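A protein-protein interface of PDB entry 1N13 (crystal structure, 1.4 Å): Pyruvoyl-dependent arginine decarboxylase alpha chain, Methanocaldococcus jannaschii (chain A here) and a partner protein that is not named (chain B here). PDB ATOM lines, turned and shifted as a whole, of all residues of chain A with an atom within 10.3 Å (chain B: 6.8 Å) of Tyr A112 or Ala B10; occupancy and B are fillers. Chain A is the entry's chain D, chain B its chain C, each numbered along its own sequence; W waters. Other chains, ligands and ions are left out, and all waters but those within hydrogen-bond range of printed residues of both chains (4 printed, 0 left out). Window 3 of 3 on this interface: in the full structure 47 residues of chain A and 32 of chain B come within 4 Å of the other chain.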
ATOM      1  N   PRO A   4     -18.788 -12.250 -12.724  1.00  0.00           N
ATOM      2  CA  PRO A   4     -19.092 -12.940 -13.984  1.00  0.00           C
ATOM      3  C   PRO A   4     -18.610 -14.390 -14.025  1.00  0.00           C
ATOM      4  O   PRO A   4     -17.596 -14.736 -13.420  1.00  0.00           O
ATOM      5  CB  PRO A   4     -18.372 -12.077 -15.023  1.00  0.00           C
ATOM      6  CG  PRO A   4     -18.439 -10.710 -14.428  1.00  0.00           C
ATOM      7  CD  PRO A   4     -18.075 -10.987 -12.984  1.00  0.00           C
ATOM      8  N   ALA A   7     -14.883 -15.893 -14.044  1.00  0.00           N
ATOM      9  CA  ALA A   7     -13.997 -14.865 -13.509  1.00  0.00           C
ATOM     10  C   ALA A   7     -13.219 -15.492 -12.358  1.00  0.00           C
ATOM     11  O   ALA A   7     -13.646 -16.489 -11.775  1.00  0.00           O
ATOM     12  CB  ALA A   7     -14.790 -13.664 -13.021  1.00  0.00           C
ATOM     13  N   GLU A   8     -12.068 -14.918 -12.039  1.00  0.00           N
ATOM     14  CA  GLU A   8     -11.244 -15.450 -10.967  1.00  0.00           C
ATOM     15  C   GLU A   8     -10.957 -14.405  -9.906  1.00  0.00           C
ATOM     16  O   GLU A   8     -10.846 -13.213 -10.212  1.00  0.00           O
ATOM     17  CB  GLU A   8      -9.911 -15.949 -11.531  1.00  0.00           C
ATOM     18  CG  GLU A   8     -10.011 -17.098 -12.539  1.00  0.00           C
ATOM     19  CD  GLU A   8     -10.451 -18.415 -11.913  1.00  0.00           C
ATOM     20  OE1 GLU A   8      -9.963 -18.753 -10.812  1.00  0.00           O
ATOM     21  OE2 GLU A   8     -11.280 -19.118 -12.532  1.00  0.00           O
ATOM     22  N   VAL A  10      -8.478 -12.721  -7.750  1.00  0.00           N
ATOM     23  CA  VAL A  10      -7.040 -12.530  -7.875  1.00  0.00           C
ATOM     24  C   VAL A  10      -6.588 -11.385  -6.990  1.00  0.00           C
ATOM     25  O   VAL A  10      -7.405 -10.582  -6.529  1.00  0.00           O
ATOM     26  CB  VAL A  10      -6.649 -12.169  -9.340  1.00  0.00           C
ATOM     27  CG1 VAL A  10      -7.081 -13.267 -10.306  1.00  0.00           C
ATOM     28  CG2 VAL A  10      -7.266 -10.828  -9.744  1.00  0.00           C
ATOM     29  N   PRO A  11      -5.282 -11.328  -6.683  1.00  0.00           N
ATOM     30  CA  PRO A  11      -4.806 -10.225  -5.843  1.00  0.00           C
ATOM     31  C   PRO A  11      -5.034  -8.947  -6.654  1.00  0.00           C
ATOM     32  O   PRO A  11      -5.092  -9.006  -7.885  1.00  0.00           O
ATOM     33  CB  PRO A  11      -3.315 -10.532  -5.704  1.00  0.00           C
ATOM     34  CG  PRO A  11      -3.278 -12.034  -5.753  1.00  0.00           C
ATOM     35  CD  PRO A  11      -4.225 -12.334  -6.890  1.00  0.00           C
ATOM     36  N   LEU A  12      -5.188  -7.811  -5.983  1.00  0.00           N
ATOM     37  CA  LEU A  12      -5.420  -6.549  -6.683  1.00  0.00           C
ATOM     38  C   LEU A  12      -4.333  -6.320  -7.726  1.00  0.00           C
ATOM     39  O   LEU A  12      -3.140  -6.351  -7.409  1.00  0.00           O
ATOM     40  CB  LEU A  12      -5.438  -5.380  -5.694  1.00  0.00           C
ATOM     41  CG  LEU A  12      -5.926  -4.035  -6.244  1.00  0.00           C
ATOM     42  CD1 LEU A  12      -7.427  -4.110  -6.516  1.00  0.00           C
ATOM     43  CD2 LEU A  12      -5.623  -2.924  -5.246  1.00  0.00           C
ATOM     44  N   PRO A  13      -4.726  -6.152  -8.999  1.00  0.00           N
ATOM     45  CA  PRO A  13      -3.740  -5.923 -10.058  1.00  0.00           C
ATOM     46  C   PRO A  13      -3.228  -4.487 -10.020  1.00  0.00           C
ATOM     47  O   PRO A  13      -3.709  -3.669  -9.233  1.00  0.00           O
ATOM     48  CB  PRO A  13      -4.549  -6.184 -11.326  1.00  0.00           C
ATOM     49  CG  PRO A  13      -5.909  -5.686 -10.951  1.00  0.00           C
ATOM     50  CD  PRO A  13      -6.088  -6.254  -9.559  1.00  0.00           C
ATOM     51  N   LYS A  14      -2.221  -4.196 -10.834  1.00  0.00           N
ATOM     52  CA  LYS A  14      -1.684  -2.845 -10.909  1.00  0.00           C
ATOM     53  C   LYS A  14      -2.712  -2.050 -11.722  1.00  0.00           C
ATOM     54  O   LYS A  14      -2.811  -2.216 -12.933  1.00  0.00           O
ATOM     55  CB  LYS A  14      -0.327  -2.848 -11.621  1.00  0.00           C
ATOM     56  CG  LYS A  14       0.386  -1.506 -11.601  1.00  0.00           C
ATOM     57  CD  LYS A  14       1.726  -1.583 -12.317  1.00  0.00           C
ATOM     58  CE  LYS A  14       2.538  -0.307 -12.132  1.00  0.00           C
ATOM     59  NZ  LYS A  14       1.865   0.903 -12.684  1.00  0.00           N
ATOM     60  N   LEU A  15      -3.507  -1.233 -11.040  1.00  0.00           N
ATOM     61  CA  LEU A  15      -4.544  -0.446 -11.703  1.00  0.00           C
ATOM     62  C   LEU A  15      -4.057   0.890 -12.243  1.00  0.00           C
ATOM     63  O   LEU A  15      -3.303   1.606 -11.580  1.00  0.00           O
ATOM     64  CB  LEU A  15      -5.719  -0.207 -10.749  1.00  0.00           C
ATOM     65  CG  LEU A  15      -6.522  -1.419 -10.274  1.00  0.00           C
ATOM     66  CD1 LEU A  15      -7.447  -1.020  -9.145  1.00  0.00           C
ATOM     67  CD2 LEU A  15      -7.311  -2.019 -11.424  1.00  0.00           C
ATOM     68  N   PRO A  16      -4.477   1.241 -13.470  1.00  0.00           N
ATOM     69  CA  PRO A  16      -4.081   2.511 -14.085  1.00  0.00           C
ATOM     70  C   PRO A  16      -4.779   3.592 -13.276  1.00  0.00           C
ATOM     71  O   PRO A  16      -5.968   3.465 -12.992  1.00  0.00           O
ATOM     72  CB  PRO A  16      -4.705   2.428 -15.482  1.00  0.00           C
ATOM     73  CG  PRO A  16      -4.915   0.957 -15.709  1.00  0.00           C
ATOM     74  CD  PRO A  16      -5.343   0.463 -14.371  1.00  0.00           C
ATOM     75  N   ALA A  19      -8.706   4.796 -13.464  1.00  0.00           N
ATOM     76  CA  ALA A  19      -9.538   3.763 -14.080  1.00  0.00           C
ATOM     77  C   ALA A  19     -10.952   3.766 -13.503  1.00  0.00           C
ATOM     78  O   ALA A  19     -11.154   4.075 -12.326  1.00  0.00           O
ATOM     79  CB  ALA A  19      -8.902   2.390 -13.896  1.00  0.00           C
ATOM     80  N   LEU A  20     -11.928   3.456 -14.352  1.00  0.00           N
ATOM     81  CA  LEU A  20     -13.334   3.395 -13.943  1.00  0.00           C
ATOM     82  C   LEU A  20     -13.577   1.948 -13.526  1.00  0.00           C
ATOM     83  O   LEU A  20     -13.995   1.114 -14.325  1.00  0.00           O
ATOM     84  CB  LEU A  20     -14.234   3.765 -15.117  1.00  0.00           C
ATOM     85  CG  LEU A  20     -13.896   5.085 -15.822  1.00  0.00           C
ATOM     86  CD1 LEU A  20     -14.800   5.262 -17.026  1.00  0.00           C
ATOM     87  CD2 LEU A  20     -14.050   6.260 -14.862  1.00  0.00           C
ATOM     88  N   VAL A  21     -13.324   1.669 -12.255  1.00  0.00           N
ATOM     89  CA  VAL A  21     -13.437   0.316 -11.726  1.00  0.00           C
ATOM     90  C   VAL A  21     -14.791  -0.037 -11.126  1.00  0.00           C
ATOM     91  O   VAL A  21     -15.222   0.579 -10.145  1.00  0.00           O
ATOM     92  CB  VAL A  21     -12.338   0.074 -10.660  1.00  0.00           C
ATOM     93  CG1 VAL A  21     -12.373  -1.366 -10.173  1.00  0.00           C
ATOM     94  CG2 VAL A  21     -10.957   0.407 -11.237  1.00  0.00           C
ATOM     95  N   PRO A  22     -15.493  -1.021 -11.727  1.00  0.00           N
ATOM     96  CA  PRO A  22     -16.805  -1.448 -11.220  1.00  0.00           C
ATOM     97  C   PRO A  22     -16.481  -2.066  -9.863  1.00  0.00           C
ATOM     98  O   PRO A  22     -15.697  -3.012  -9.781  1.00  0.00           O
ATOM     99  CB  PRO A  22     -17.238  -2.516 -12.232  1.00  0.00           C
ATOM    100  CG  PRO A  22     -16.501  -2.139 -13.485  1.00  0.00           C
ATOM    101  CD  PRO A  22     -15.143  -1.754 -12.956  1.00  0.00           C
ATOM    102  N   ALA A 109     -13.399  -5.322  -6.192  1.00  0.00           N
ATOM    103  CA  ALA A 109     -13.142  -4.591  -7.427  1.00  0.00           C
ATOM    104  C   ALA A 109     -13.053  -5.525  -8.624  1.00  0.00           C
ATOM    105  O   ALA A 109     -12.270  -6.476  -8.628  1.00  0.00           O
ATOM    106  CB  ALA A 109     -11.857  -3.785  -7.291  1.00  0.00           C
ATOM    107  N   LEU A 110     -13.865  -5.247  -9.637  1.00  0.00           N
ATOM    108  CA  LEU A 110     -13.883  -6.050 -10.850  1.00  0.00           C
ATOM    109  C   LEU A 110     -12.937  -5.444 -11.880  1.00  0.00           C
ATOM    110  O   LEU A 110     -12.976  -4.242 -12.135  1.00  0.00           O
ATOM    111  CB  LEU A 110     -15.308  -6.114 -11.421  1.00  0.00           C
ATOM    112  CG  LEU A 110     -16.357  -6.991 -10.720  1.00  0.00           C
ATOM    113  CD1 LEU A 110     -16.580  -6.542  -9.285  1.00  0.00           C
ATOM    114  CD2 LEU A 110     -17.666  -6.943 -11.502  1.00  0.00           C
ATOM    115  N   TRP A 111     -12.040  -6.256 -12.433  1.00  0.00           N
ATOM    116  CA  TRP A 111     -11.125  -5.733 -13.437  1.00  0.00           C
ATOM    117  C   TRP A 111     -10.785  -6.754 -14.518  1.00  0.00           C
ATOM    118  O   TRP A 111     -11.552  -7.694 -14.747  1.00  0.00           O
ATOM    119  CB  TRP A 111      -9.874  -5.107 -12.793  1.00  0.00           C
ATOM    120  CG  TRP A 111      -9.162  -4.116 -13.683  1.00  0.00           C
ATOM    121  CD1 TRP A 111      -7.862  -4.183 -14.102  1.00  0.00           C
ATOM    122  CD2 TRP A 111      -9.719  -2.939 -14.296  1.00  0.00           C
ATOM    123  NE1 TRP A 111      -7.576  -3.129 -14.941  1.00  0.00           N
ATOM    124  CE2 TRP A 111      -8.696  -2.352 -15.077  1.00  0.00           C
ATOM    125  CE3 TRP A 111     -10.981  -2.327 -14.264  1.00  0.00           C
ATOM    126  CZ2 TRP A 111      -8.895  -1.184 -15.823  1.00  0.00           C
ATOM    127  CZ3 TRP A 111     -11.180  -1.161 -15.006  1.00  0.00           C
ATOM    128  CH2 TRP A 111     -10.140  -0.605 -15.776  1.00  0.00           C
ATOM    129  N   TYR A 112      -9.641  -6.579 -15.175  1.00  0.00           N
ATOM    130  CA  TYR A 112      -9.262  -7.449 -16.282  1.00  0.00           C
ATOM    131  C   TYR A 112      -7.893  -8.100 -16.169  1.00  0.00           C
ATOM    132  O   TYR A 112      -6.971  -7.510 -15.620  1.00  0.00           O
ATOM    133  CB  TYR A 112      -9.315  -6.644 -17.586  1.00  0.00           C
ATOM    134  CG  TYR A 112     -10.668  -6.054 -17.891  1.00  0.00           C
ATOM    135  CD1 TYR A 112     -11.524  -6.676 -18.789  1.00  0.00           C
ATOM    136  CD2 TYR A 112     -11.098  -4.873 -17.278  1.00  0.00           C
ATOM    137  CE1 TYR A 112     -12.778  -6.146 -19.074  1.00  0.00           C
ATOM    138  CE2 TYR A 112     -12.353  -4.335 -17.553  1.00  0.00           C
ATOM    139  CZ  TYR A 112     -13.183  -4.978 -18.451  1.00  0.00           C
ATOM    140  OH  TYR A 112     -14.427  -4.469 -18.715  1.00  0.00           O
ATOM    141  N   LYS A 113      -7.774  -9.299 -16.739  1.00  0.00           N
ATOM    142  CA  LYS A 113      -6.522 -10.063 -16.753  1.00  0.00           C
ATOM    143  C   LYS A 113      -5.459  -9.345 -17.583  1.00  0.00           C
ATOM    144  O   LYS A 113      -4.271  -9.410 -17.201  1.00  0.00           O
ATOM    145  CB  LYS A 113      -6.741 -11.450 -17.368  1.00  0.00           C
ATOM    146  CG  LYS A 113      -7.568 -12.411 -16.545  1.00  0.00           C
ATOM    147  CD  LYS A 113      -7.688 -13.761 -17.254  1.00  0.00           C
ATOM    148  CE  LYS A 113      -8.384 -13.631 -18.604  1.00  0.00           C
ATOM    149  NZ  LYS A 113      -8.529 -14.938 -19.305  1.00  0.00           N
ATOM    150  OXT LYS A 113      -5.822  -8.761 -18.628  1.00  0.00           O
ATOM    151  N   PRO B   7      -6.677 -12.756 -27.280  1.00  0.00           N
ATOM    152  CA  PRO B   7      -7.855 -11.882 -27.263  1.00  0.00           C
ATOM    153  C   PRO B   7      -7.517 -10.395 -27.373  1.00  0.00           C
ATOM    154  O   PRO B   7      -6.587  -9.907 -26.727  1.00  0.00           O
ATOM    155  CB  PRO B   7      -8.492 -12.199 -25.908  1.00  0.00           C
ATOM    156  CG  PRO B   7      -8.085 -13.618 -25.662  1.00  0.00           C
ATOM    157  CD  PRO B   7      -6.636 -13.594 -26.069  1.00  0.00           C
ATOM    158  N   LEU B   8      -8.257  -9.696 -28.229  1.00  0.00           N
ATOM    159  CA  LEU B   8      -8.087  -8.259 -28.427  1.00  0.00           C
ATOM    160  C   LEU B   8      -9.363  -7.582 -27.936  1.00  0.00           C
ATOM    161  O   LEU B   8     -10.394  -8.240 -27.785  1.00  0.00           O
ATOM    162  CB  LEU B   8      -7.864  -7.935 -29.907  1.00  0.00           C
ATOM    163  CG  LEU B   8      -6.626  -8.538 -30.575  1.00  0.00           C
ATOM    164  CD1 LEU B   8      -6.674  -8.264 -32.063  1.00  0.00           C
ATOM    165  CD2 LEU B   8      -5.356  -7.965 -29.968  1.00  0.00           C
ATOM    166  N   HIS B   9      -9.295  -6.276 -27.691  1.00  0.00           N
ATOM    167  CA  HIS B   9     -10.447  -5.512 -27.204  1.00  0.00           C
ATOM    168  C   HIS B   9     -11.023  -6.116 -25.930  1.00  0.00           C
ATOM    169  O   HIS B   9     -12.229  -6.041 -25.684  1.00  0.00           O
ATOM    170  CB  HIS B   9     -11.538  -5.417 -28.274  1.00  0.00           C
ATOM    171  CG  HIS B   9     -11.231  -4.436 -29.361  1.00  0.00           C
ATOM    172  ND1 HIS B   9     -11.695  -4.582 -30.650  1.00  0.00           N
ATOM    173  CD2 HIS B   9     -10.512  -3.288 -29.348  1.00  0.00           C
ATOM    174  CE1 HIS B   9     -11.275  -3.567 -31.384  1.00  0.00           C
ATOM    175  NE2 HIS B   9     -10.556  -2.768 -30.617  1.00  0.00           N
ATOM    176  N   ALA B  10     -10.148  -6.714 -25.125  1.00  0.00           N
ATOM    177  CA  ALA B  10     -10.551  -7.343 -23.874  1.00  0.00           C
ATOM    178  C   ALA B  10     -11.188  -6.350 -22.904  1.00  0.00           C
ATOM    179  O   ALA B  10     -12.155  -6.683 -22.221  1.00  0.00           O
ATOM    180  CB  ALA B  10      -9.356  -8.027 -23.221  1.00  0.00           C
ATOM    181  N   TYR B  11     -10.669  -5.124 -22.870  1.00  0.00           N
ATOM    182  CA  TYR B  11     -11.203  -4.106 -21.965  1.00  0.00           C
ATOM    183  C   TYR B  11     -12.602  -3.612 -22.319  1.00  0.00           C
ATOM    184  O   TYR B  11     -13.253  -2.951 -21.509  1.00  0.00           O
ATOM    185  CB  TYR B  11     -10.236  -2.931 -21.842  1.00  0.00           C
ATOM    186  CG  TYR B  11      -9.030  -3.248 -20.997  1.00  0.00           C
ATOM    187  CD1 TYR B  11      -9.003  -2.922 -19.645  1.00  0.00           C
ATOM    188  CD2 TYR B  11      -7.925  -3.899 -21.541  1.00  0.00           C
ATOM    189  CE1 TYR B  11      -7.909  -3.236 -18.850  1.00  0.00           C
ATOM    190  CE2 TYR B  11      -6.821  -4.221 -20.754  1.00  0.00           C
ATOM    191  CZ  TYR B  11      -6.823  -3.886 -19.410  1.00  0.00           C
ATOM    192  OH  TYR B  11      -5.747  -4.209 -18.620  1.00  0.00           O
ATOM    193  N   PHE B  12     -13.069  -3.941 -23.521  1.00  0.00           N
ATOM    194  CA  PHE B  12     -14.404  -3.535 -23.950  1.00  0.00           C
ATOM    195  C   PHE B  12     -15.449  -4.582 -23.605  1.00  0.00           C
ATOM    196  O   PHE B  12     -16.645  -4.364 -23.788  1.00  0.00           O
ATOM    197  CB  PHE B  12     -14.422  -3.244 -25.450  1.00  0.00           C
ATOM    198  CG  PHE B  12     -13.701  -1.988 -25.820  1.00  0.00           C
ATOM    199  CD1 PHE B  12     -14.161  -0.755 -25.372  1.00  0.00           C
ATOM    200  CD2 PHE B  12     -12.552  -2.032 -26.599  1.00  0.00           C
ATOM    201  CE1 PHE B  12     -13.489   0.413 -25.693  1.00  0.00           C
ATOM    202  CE2 PHE B  12     -11.871  -0.867 -26.926  1.00  0.00           C
ATOM    203  CZ  PHE B  12     -12.339   0.360 -26.473  1.00  0.00           C
ATOM    204  N   LYS B  13     -14.982  -5.722 -23.109  1.00  0.00           N
ATOM    205  CA  LYS B  13     -15.857  -6.814 -22.721  1.00  0.00           C
ATOM    206  C   LYS B  13     -16.073  -6.790 -21.212  1.00  0.00           C
ATOM    207  O   LYS B  13     -15.723  -5.814 -20.549  1.00  0.00           O
ATOM    208  CB  LYS B  13     -15.262  -8.145 -23.174  1.00  0.00           C
ATOM    209  CG  LYS B  13     -15.132  -8.256 -24.684  1.00  0.00           C
ATOM    210  CD  LYS B  13     -14.502  -9.571 -25.098  1.00  0.00           C
ATOM    211  CE  LYS B  13     -14.343  -9.644 -26.613  1.00  0.00           C
ATOM    212  NZ  LYS B  13     -13.484  -8.544 -27.141  1.00  0.00           N
ATOM    213  N   LEU B  14     -16.663  -7.854 -20.678  1.00  0.00           N
ATOM    214  CA  LEU B  14     -16.940  -7.945 -19.246  1.00  0.00           C
ATOM    215  C   LEU B  14     -15.687  -8.215 -18.416  1.00  0.00           C
ATOM    216  O   LEU B  14     -14.768  -8.910 -18.867  1.00  0.00           O
ATOM    217  CB  LEU B  14     -17.956  -9.061 -18.986  1.00  0.00           C
ATOM    218  CG  LEU B  14     -19.400  -8.702 -18.626  1.00  0.00           C
ATOM    219  CD1 LEU B  14     -19.890  -7.512 -19.416  1.00  0.00           C
ATOM    220  CD2 LEU B  14     -20.288  -9.920 -18.832  1.00  0.00           C
ATOM    221  N   PRO B  15     -15.614  -7.634 -17.203  1.00  0.00           N
ATOM    222  CA  PRO B  15     -14.449  -7.856 -16.339  1.00  0.00           C
ATOM    223  C   PRO B  15     -14.321  -9.353 -16.068  1.00  0.00           C
ATOM    224  O   PRO B  15     -15.327 -10.056 -15.974  1.00  0.00           O
ATOM    225  CB  PRO B  15     -14.835  -7.111 -15.061  1.00  0.00           C
ATOM    226  CG  PRO B  15     -15.637  -5.972 -15.574  1.00  0.00           C
ATOM    227  CD  PRO B  15     -16.520  -6.633 -16.610  1.00  0.00           C
ATOM    228  N   ASN B  16     -13.093  -9.844 -15.964  1.00  0.00           N
ATOM    229  CA  ASN B  16     -12.883 -11.264 -15.715  1.00  0.00           C
ATOM    230  C   ASN B  16     -12.102 -11.586 -14.447  1.00  0.00           C
ATOM    231  O   ASN B  16     -11.642 -12.712 -14.274  1.00  0.00           O
ATOM    232  CB  ASN B  16     -12.246 -11.942 -16.932  1.00  0.00           C
ATOM    233  CG  ASN B  16     -11.028 -11.205 -17.443  1.00  0.00           C
ATOM    234  OD1 ASN B  16     -10.313 -10.557 -16.685  1.00  0.00           O
ATOM    235  ND2 ASN B  16     -10.791 -11.296 -18.745  1.00  0.00           N
ATOM    236  N   THR B  17     -11.921 -10.590 -13.582  1.00  0.00           N
ATOM    237  CA  THR B  17     -11.232 -10.795 -12.308  1.00  0.00           C
ATOM    238  C   THR B  17     -11.935  -9.988 -11.225  1.00  0.00           C
ATOM    239  O   THR B  17     -12.588  -8.979 -11.510  1.00  0.00           O
ATOM    240  CB  THR B  17      -9.736 -10.357 -12.318  1.00  0.00           C
ATOM    241  OG1 THR B  17      -9.641  -8.933 -12.407  1.00  0.00           O
ATOM    242  CG2 THR B  17      -8.969 -11.000 -13.468  1.00  0.00           C
HETATM  243  O   HOH W   1      -5.050  -2.648 -16.433  1.00  0.00           O
HETATM  244  O   HOH W   2      -9.902  -7.471  -9.936  1.00  0.00           O
HETATM  245  O   HOH W   3      -7.086  -8.112 -12.931  1.00  0.00           O
HETATM  246  O   HOH W   4      -8.602  -9.403 -19.929  1.00  0.00           O
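CG of Pro A4 touches O of Pro B15 (3.5 Å).
Leu A110 touches Pro B15 (CB to CB, 3.8 Å).
CA of Leu A110 touches O of Thr B17 (3.3 Å).
Tyr B11 touches Trp A111.
CA of Pro B15 touches O of Trp A111, at 3.3 Å.
O of Ala B10 touches CE1 of Tyr A112, at 3.3 Å.
CE1 of Tyr A112 touches O of Leu B14 (3.4 Å).
CE1 of Tyr A112 touches CA of Pro B15 (3.6 Å).
Tyr A112 touches Asn B16.
Lys A113 touches Thr B17.
Printed residues of chain B within 4 Å of Glu A8: Asn B16 (3.2 Å) and Thr B17 (3.2 Å).
Printed residues of chain B within 4 Å of Val A10: Thr B17.
Leu A15 touches none of the printed residues of chain B.
Pro A22 touches none of the printed residues of chain B.
Of the printed residues of chain B, Ala A109 touches Thr B17 (3.8 Å).
Of chain B, only Ala B10 (3.3 Å), Tyr B11 (3.4 Å), Lys B13 (2.6 Å), Leu B14 (3.4 Å), Pro B15 (3.6 Å), Asn B16 (3.3 Å) and Thr B17 (3.6 Å) come within 4 Å of Tyr A112.
Of the printed residues of chain B, Lys A113 touches Asn B16 (2.8 Å) and Thr B17 (3.7 Å).
Of chain A, only Tyr A112 (3.3 Å) comes within 4 Å of Ala B10.
Of the printed residues of chain A, Lys B13 touches Tyr A112.
Pro B15 touches just these residues of chain A: Pro A4, Leu A110, Trp A111 and Tyr A112.
Of chain A, only Ala A7 (3.3 Å), Glu A8 (3.2 Å), Trp A111 (2.9 Å), Tyr A112 (3.3 Å) and Lys A113 (2.8 Å) come within 4 Å of Asn B16.
The nearest residue of chain B that does not touch Tyr A112 is Phe B12 (5.0 Å).
The nearest residue of chain A that does not touch Ala B10 is Lys A113 (5.8 Å).
Hydrophobic or aromatic side chains of chain A that line the printed part of chain B: Pro A4, Ala A7, Val A10, Leu A110, Trp A111 and Tyr A112.
Of the 11 printed residues of chain B, 7 touch a printed residue of chain A.
Printed residues of chain B that touch a printed residue of chain A: Ala B10, Tyr B11, Lys B13, Leu B14, Pro B15, Asn B16 and Thr B17.
Hydrophobic or aromatic side chains of chain B within 4 Å of the printed part of chain A: Tyr B11 and Pro B15.
Among the printed residues, no Asp or Glu carboxylate lies within 4 Å of a Lys or Arg side-chain nitrogen of the other chain.
The backbone carbonyl oxygen of Pro A22 is in hydrogen-bond range of the backbone NH of Leu A110 (2.9 Å).
The backbone carbonyl oxygen (O) of His B9 lies within hydrogen-bond range of the side-chain amino group (NZ) of Lys B13 (3.2 Å).
The backbone carbonyl oxygen of Leu B8 is in hydrogen-bond range of the side-chain amino group of Lys B13 (3.2 Å).
Water W3 bridges OG1 of Thr B17 (2.7 Å) and O of Tyr A112 (2.8 Å).
Water W1 bridges the side-chain hydroxyl of Tyr B11 (2.8 Å) and the indole nitrogen of Trp A111 (3.0 Å).
Water W2 lies within hydrogen-bond range of the backbone carbonyl oxygen (O) of Ala A109 (2.9 Å) and the side-chain hydroxyl (OG1) of Thr B17 (2.9 Å).
Water W4 bridges the side-chain amide nitrogen of Asn B16 (3.1 Å) and the chain-end carboxylate of Lys A113 (3.1 Å).
N of Lys A113 sits at hydrogen-bond distance from OD1 of Asn B16 (2.8 Å).
The backbone carbonyl oxygen (O) of Asn B16 sits at hydrogen-bond distance from the backbone NH (N) of Glu A8, at 3.2 Å.
The backbone NH (N) of Trp A111 is in hydrogen-bond range of the backbone carbonyl oxygen (O) of Thr B17, at 2.9 Å.
The backbone carbonyl oxygen (O) of Trp A111 sits at hydrogen-bond distance from the backbone NH (N) of Asn B16 (2.9 Å).
The backbone carbonyl oxygen (O) of Tyr B11 sits at hydrogen-bond distance from the side-chain hydroxyl (OH) of Tyr A112, 3.4 Å away.
OH of Tyr A112 lies within hydrogen-bond range of O of Lys B13 (2.6 Å).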
